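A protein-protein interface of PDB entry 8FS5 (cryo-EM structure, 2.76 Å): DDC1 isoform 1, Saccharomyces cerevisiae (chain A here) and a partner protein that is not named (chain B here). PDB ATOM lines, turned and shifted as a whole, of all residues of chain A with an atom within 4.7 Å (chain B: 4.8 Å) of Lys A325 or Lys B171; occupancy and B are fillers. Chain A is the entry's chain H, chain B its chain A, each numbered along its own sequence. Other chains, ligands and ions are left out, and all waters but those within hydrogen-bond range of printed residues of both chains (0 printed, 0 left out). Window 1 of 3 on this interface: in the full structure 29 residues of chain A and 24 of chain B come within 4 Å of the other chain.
Among the printed residues, merely in contact across the chains: Phe A324 with Tyr B175 (3.7 Å), Lys A327 with Glu B168 (3.9 Å), Lys A325 with Tyr B175 (3.97 Å) and Lys A325 with Lys B171 (3.99 Å).
Printed residues of chain A within 4 Å of Lys B171: Asp A250 (3.4 Å) and Lys A325 (3.99 Å). Of the printed residues of chain B, Phe A324 touches Tyr B175. Printed residues of chain B within 4 Å of Asp A250: Lys B171. Printed residues of chain A within 4 Å of Tyr B175: Phe A324 and Lys A325. Of the printed residues of chain A, Glu B168 touches Lys A325 and Lys A327. The nearest printed residue of chain B that does not touch Lys A325 is Gly B172 (4.3 Å). The nearest printed residue of chain A that does not touch Lys B171 is Arg A279 (4.6 Å).
OE1 of Glu B168 lies within salt-bridge range of NZ of Lys A325 (3.0 Å). NZ of Lys B171 lies within salt-bridge range of OD2 of Asp A250 (3.7 Å).
Hydrophobic or aromatic side chains of chain B within 4 Å of the printed part of chain A: Tyr B175.
OG of Ser B167 lies within hydrogen-bond range of NZ of Lys B171, at 2.7 Å. The side-chain carboxylate (OD2) of Asp A250 lies within salt-bridge range of the guanidinium group (NH1) of Arg A279 (3.96 Å). O of Asp A250 sits at hydrogen-bond distance from N of Leu A326 (3.1 Å). O of Phe A324 is in hydrogen-bond range of N of Val A252. N of Lys A325 is in hydrogen-bond range of OE1 of Glu A375, at 3.3 Å.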
ATOM      1  N   ASP A 250      -2.272  28.581 -25.252  1.00  0.00           N
ATOM      2  CA  ASP A 250      -2.185  27.366 -24.450  1.00  0.00           C
ATOM      3  C   ASP A 250      -0.965  27.319 -23.546  1.00  0.00           C
ATOM      4  O   ASP A 250      -1.069  26.859 -22.407  1.00  0.00           O
ATOM      5  CB  ASP A 250      -2.180  26.132 -25.363  1.00  0.00           C
ATOM      6  CG  ASP A 250      -3.358  26.106 -26.313  1.00  0.00           C
ATOM      7  OD1 ASP A 250      -4.498  26.324 -25.855  1.00  0.00           O
ATOM      8  OD2 ASP A 250      -3.147  25.857 -27.516  1.00  0.00           O
ATOM      9  N   VAL A 252       2.463  29.032 -21.552  1.00  0.00           N
ATOM     10  CA  VAL A 252       2.961  30.241 -20.909  1.00  0.00           C
ATOM     11  C   VAL A 252       4.450  30.069 -20.641  1.00  0.00           C
ATOM     12  O   VAL A 252       4.873  29.058 -20.066  1.00  0.00           O
ATOM     13  CB  VAL A 252       2.191  30.554 -19.611  1.00  0.00           C
ATOM     14  CG1 VAL A 252       2.029  29.306 -18.756  1.00  0.00           C
ATOM     15  CG2 VAL A 252       2.889  31.656 -18.826  1.00  0.00           C
ATOM     16  N   ARG A 279      -2.334  25.992 -37.939  1.00  0.00           N
ATOM     17  CA  ARG A 279      -2.591  26.742 -36.720  1.00  0.00           C
ATOM     18  C   ARG A 279      -1.687  27.965 -36.681  1.00  0.00           C
ATOM     19  O   ARG A 279      -0.511  27.889 -37.047  1.00  0.00           O
ATOM     20  CB  ARG A 279      -2.366  25.877 -35.474  1.00  0.00           C
ATOM     21  CG  ARG A 279      -2.898  26.488 -34.192  1.00  0.00           C
ATOM     22  CD  ARG A 279      -3.299  25.413 -33.200  1.00  0.00           C
ATOM     23  NE  ARG A 279      -3.505  25.956 -31.864  1.00  0.00           N
ATOM     24  CZ  ARG A 279      -2.616  25.883 -30.883  1.00  0.00           C
ATOM     25  NH1 ARG A 279      -1.449  25.284 -31.050  1.00  0.00           N
ATOM     26  NH2 ARG A 279      -2.904  26.431 -29.706  1.00  0.00           N
ATOM     27  N   PHE A 324       4.681  25.806 -19.398  1.00  0.00           N
ATOM     28  CA  PHE A 324       3.654  24.905 -18.889  1.00  0.00           C
ATOM     29  C   PHE A 324       2.298  25.363 -19.414  1.00  0.00           C
ATOM     30  O   PHE A 324       2.198  26.323 -20.184  1.00  0.00           O
ATOM     31  CB  PHE A 324       3.677  24.828 -17.355  1.00  0.00           C
ATOM     32  CG  PHE A 324       3.660  26.167 -16.664  1.00  0.00           C
ATOM     33  CD1 PHE A 324       4.822  26.909 -16.515  1.00  0.00           C
ATOM     34  CD2 PHE A 324       2.479  26.675 -16.148  1.00  0.00           C
ATOM     35  CE1 PHE A 324       4.802  28.134 -15.875  1.00  0.00           C
ATOM     36  CE2 PHE A 324       2.454  27.899 -15.506  1.00  0.00           C
ATOM     37  CZ  PHE A 324       3.618  28.629 -15.370  1.00  0.00           C
ATOM     38  N   LYS A 325       1.248  24.661 -18.993  1.00  0.00           N
ATOM     39  CA  LYS A 325      -0.091  24.906 -19.502  1.00  0.00           C
ATOM     40  C   LYS A 325      -0.688  26.170 -18.885  1.00  0.00           C
ATOM     41  O   LYS A 325      -0.155  26.749 -17.936  1.00  0.00           O
ATOM     42  CB  LYS A 325      -0.995  23.704 -19.234  1.00  0.00           C
ATOM     43  CG  LYS A 325      -0.694  22.497 -20.109  1.00  0.00           C
ATOM     44  CD  LYS A 325      -1.933  21.639 -20.326  1.00  0.00           C
ATOM     45  CE  LYS A 325      -3.136  22.485 -20.719  1.00  0.00           C
ATOM     46  NZ  LYS A 325      -4.112  21.718 -21.540  1.00  0.00           N
ATOM     47  N   LEU A 326      -1.821  26.595 -19.444  1.00  0.00           N
ATOM     48  CA  LEU A 326      -2.464  27.844 -19.060  1.00  0.00           C
ATOM     49  C   LEU A 326      -3.867  27.676 -18.497  1.00  0.00           C
ATOM     50  O   LEU A 326      -4.301  28.520 -17.711  1.00  0.00           O
ATOM     51  CB  LEU A 326      -2.534  28.797 -20.264  1.00  0.00           C
ATOM     52  CG  LEU A 326      -2.669  30.286 -19.951  1.00  0.00           C
ATOM     53  CD1 LEU A 326      -1.417  30.768 -19.254  1.00  0.00           C
ATOM     54  CD2 LEU A 326      -2.924  31.086 -21.218  1.00  0.00           C
ATOM     55  N   LYS A 327      -4.588  26.617 -18.876  1.00  0.00           N
ATOM     56  CA  LYS A 327      -5.984  26.471 -18.476  1.00  0.00           C
ATOM     57  C   LYS A 327      -6.156  26.261 -16.978  1.00  0.00           C
ATOM     58  O   LYS A 327      -7.208  26.622 -16.439  1.00  0.00           O
ATOM     59  CB  LYS A 327      -6.626  25.310 -19.238  1.00  0.00           C
ATOM     60  CG  LYS A 327      -8.136  25.427 -19.383  1.00  0.00           C
ATOM     61  CD  LYS A 327      -8.768  24.087 -19.724  1.00  0.00           C
ATOM     62  CE  LYS A 327      -8.397  23.024 -18.704  1.00  0.00           C
ATOM     63  NZ  LYS A 327      -8.908  23.356 -17.346  1.00  0.00           N
ATOM     64  N   PHE A 329      -3.494  27.232 -14.670  1.00  0.00           N
ATOM     65  CA  PHE A 329      -2.816  28.340 -14.005  1.00  0.00           C
ATOM     66  C   PHE A 329      -3.774  29.489 -13.729  1.00  0.00           C
ATOM     67  O   PHE A 329      -3.771  30.049 -12.629  1.00  0.00           O
ATOM     68  CB  PHE A 329      -1.635  28.820 -14.847  1.00  0.00           C
ATOM     69  CG  PHE A 329      -0.854  29.937 -14.215  1.00  0.00           C
ATOM     70  CD1 PHE A 329      -0.347  29.807 -12.934  1.00  0.00           C
ATOM     71  CD2 PHE A 329      -0.627  31.118 -14.902  1.00  0.00           C
ATOM     72  CE1 PHE A 329       0.372  30.834 -12.348  1.00  0.00           C
ATOM     73  CE2 PHE A 329       0.092  32.148 -14.323  1.00  0.00           C
ATOM     74  CZ  PHE A 329       0.591  32.006 -13.043  1.00  0.00           C
ATOM     75  N   GLU A 375       2.421  21.402 -11.760  1.00  0.00           N
ATOM     76  CA  GLU A 375       2.235  21.197 -13.189  1.00  0.00           C
ATOM     77  C   GLU A 375       3.531  20.703 -13.814  1.00  0.00           C
ATOM     78  O   GLU A 375       4.626  21.099 -13.408  1.00  0.00           O
ATOM     79  CB  GLU A 375       1.774  22.482 -13.891  1.00  0.00           C
ATOM     80  CG  GLU A 375       0.270  22.692 -13.872  1.00  0.00           C
ATOM     81  CD  GLU A 375      -0.209  23.561 -15.017  1.00  0.00           C
ATOM     82  OE1 GLU A 375       0.644  24.106 -15.748  1.00  0.00           O
ATOM     83  OE2 GLU A 375      -1.438  23.698 -15.189  1.00  0.00           O
ATOM     84  N   SER B 167      -8.776  17.887 -27.464  1.00  0.00           N
ATOM     85  CA  SER B 167      -7.718  18.870 -27.662  1.00  0.00           C
ATOM     86  C   SER B 167      -6.905  19.100 -26.395  1.00  0.00           C
ATOM     87  O   SER B 167      -5.671  19.126 -26.455  1.00  0.00           O
ATOM     88  CB  SER B 167      -8.313  20.192 -28.150  1.00  0.00           C
ATOM     89  OG  SER B 167      -7.297  21.098 -28.539  1.00  0.00           O
ATOM     90  N   GLU B 168      -7.564  19.246 -25.247  1.00  0.00           N
ATOM     91  CA  GLU B 168      -6.867  19.410 -23.979  1.00  0.00           C
ATOM     92  C   GLU B 168      -6.159  18.141 -23.526  1.00  0.00           C
ATOM     93  O   GLU B 168      -5.192  18.227 -22.762  1.00  0.00           O
ATOM     94  CB  GLU B 168      -7.841  19.872 -22.893  1.00  0.00           C
ATOM     95  CG  GLU B 168      -8.634  21.110 -23.267  1.00  0.00           C
ATOM     96  CD  GLU B 168      -7.754  22.329 -23.456  1.00  0.00           C
ATOM     97  OE1 GLU B 168      -6.777  22.485 -22.692  1.00  0.00           O
ATOM     98  OE2 GLU B 168      -8.037  23.133 -24.369  1.00  0.00           O
ATOM     99  N   PHE B 169      -6.608  16.971 -23.980  1.00  0.00           N
ATOM    100  CA  PHE B 169      -5.884  15.730 -23.743  1.00  0.00           C
ATOM    101  C   PHE B 169      -4.617  15.635 -24.575  1.00  0.00           C
ATOM    102  O   PHE B 169      -3.569  15.242 -24.056  1.00  0.00           O
ATOM    103  CB  PHE B 169      -6.777  14.521 -24.039  1.00  0.00           C
ATOM    104  CG  PHE B 169      -6.049  13.205 -23.984  1.00  0.00           C
ATOM    105  CD1 PHE B 169      -5.759  12.610 -22.768  1.00  0.00           C
ATOM    106  CD2 PHE B 169      -5.658  12.563 -25.149  1.00  0.00           C
ATOM    107  CE1 PHE B 169      -5.089  11.403 -22.712  1.00  0.00           C
ATOM    108  CE2 PHE B 169      -4.987  11.357 -25.100  1.00  0.00           C
ATOM    109  CZ  PHE B 169      -4.703  10.775 -23.879  1.00  0.00           C
ATOM    110  N   LEU B 170      -4.689  15.990 -25.859  1.00  0.00           N
ATOM    111  CA  LEU B 170      -3.500  16.000 -26.702  1.00  0.00           C
ATOM    112  C   LEU B 170      -2.536  17.122 -26.343  1.00  0.00           C
ATOM    113  O   LEU B 170      -1.339  16.997 -26.621  1.00  0.00           O
ATOM    114  CB  LEU B 170      -3.894  16.117 -28.175  1.00  0.00           C
ATOM    115  CG  LEU B 170      -4.134  14.811 -28.933  1.00  0.00           C
ATOM    116  CD1 LEU B 170      -4.097  15.056 -30.433  1.00  0.00           C
ATOM    117  CD2 LEU B 170      -3.118  13.752 -28.533  1.00  0.00           C
ATOM    118  N   LYS B 171      -3.023  18.204 -25.738  1.00  0.00           N
ATOM    119  CA  LYS B 171      -2.156  19.304 -25.338  1.00  0.00           C
ATOM    120  C   LYS B 171      -1.414  19.025 -24.040  1.00  0.00           C
ATOM    121  O   LYS B 171      -0.378  19.648 -23.781  1.00  0.00           O
ATOM    122  CB  LYS B 171      -2.977  20.587 -25.194  1.00  0.00           C
ATOM    123  CG  LYS B 171      -3.226  21.304 -26.509  1.00  0.00           C
ATOM    124  CD  LYS B 171      -3.724  22.715 -26.277  1.00  0.00           C
ATOM    125  CE  LYS B 171      -5.218  22.822 -26.536  1.00  0.00           C
ATOM    126  NZ  LYS B 171      -5.519  23.090 -27.970  1.00  0.00           N
ATOM    127  N   GLY B 172      -1.921  18.111 -23.216  1.00  0.00           N
ATOM    128  CA  GLY B 172      -1.230  17.718 -22.004  1.00  0.00           C
ATOM    129  C   GLY B 172      -0.464  16.424 -22.178  1.00  0.00           C
ATOM    130  O   GLY B 172       0.463  16.129 -21.417  1.00  0.00           O
ATOM    131  N   ALA B 173      -0.848  15.640 -23.189  1.00  0.00           N
ATOM    132  CA  ALA B 173      -0.146  14.393 -23.472  1.00  0.00           C
ATOM    133  C   ALA B 173       1.196  14.647 -24.142  1.00  0.00           C
ATOM    134  O   ALA B 173       2.114  13.829 -24.018  1.00  0.00           O
ATOM    135  CB  ALA B 173      -1.015  13.490 -24.345  1.00  0.00           C
ATOM    136  N   ARG B 174       1.329  15.768 -24.855  1.00  0.00           N
ATOM    137  CA  ARG B 174       2.593  16.101 -25.501  1.00  0.00           C
ATOM    138  C   ARG B 174       3.688  16.430 -24.495  1.00  0.00           C
ATOM    139  O   ARG B 174       4.867  16.448 -24.864  1.00  0.00           O
ATOM    140  CB  ARG B 174       2.389  17.267 -26.471  1.00  0.00           C
ATOM    141  CG  ARG B 174       1.925  18.549 -25.809  1.00  0.00           C
ATOM    142  CD  ARG B 174       2.629  19.757 -26.395  1.00  0.00           C
ATOM    143  NE  ARG B 174       3.922  19.983 -25.763  1.00  0.00           N
ATOM    144  CZ  ARG B 174       4.465  21.178 -25.579  1.00  0.00           C
ATOM    145  NH1 ARG B 174       3.851  22.284 -25.963  1.00  0.00           N
ATOM    146  NH2 ARG B 174       5.655  21.265 -24.993  1.00  0.00           N
ATOM    147  N   TYR B 175       3.330  16.698 -23.238  1.00  0.00           N
ATOM    148  CA  TYR B 175       4.320  16.862 -22.182  1.00  0.00           C
ATOM    149  C   TYR B 175       4.814  15.535 -21.622  1.00  0.00           C
ATOM    150  O   TYR B 175       5.745  15.536 -20.809  1.00  0.00           O
ATOM    151  CB  TYR B 175       3.754  17.715 -21.043  1.00  0.00           C
ATOM    152  CG  TYR B 175       3.570  19.174 -21.391  1.00  0.00           C
ATOM    153  CD1 TYR B 175       2.405  19.625 -21.997  1.00  0.00           C
ATOM    154  CD2 TYR B 175       4.562  20.104 -21.108  1.00  0.00           C
ATOM    155  CE1 TYR B 175       2.235  20.962 -22.313  1.00  0.00           C
ATOM    156  CE2 TYR B 175       4.403  21.440 -21.420  1.00  0.00           C
ATOM    157  CZ  TYR B 175       3.238  21.864 -22.023  1.00  0.00           C
ATOM    158  OH  TYR B 175       3.076  23.194 -22.334  1.00  0.00           O
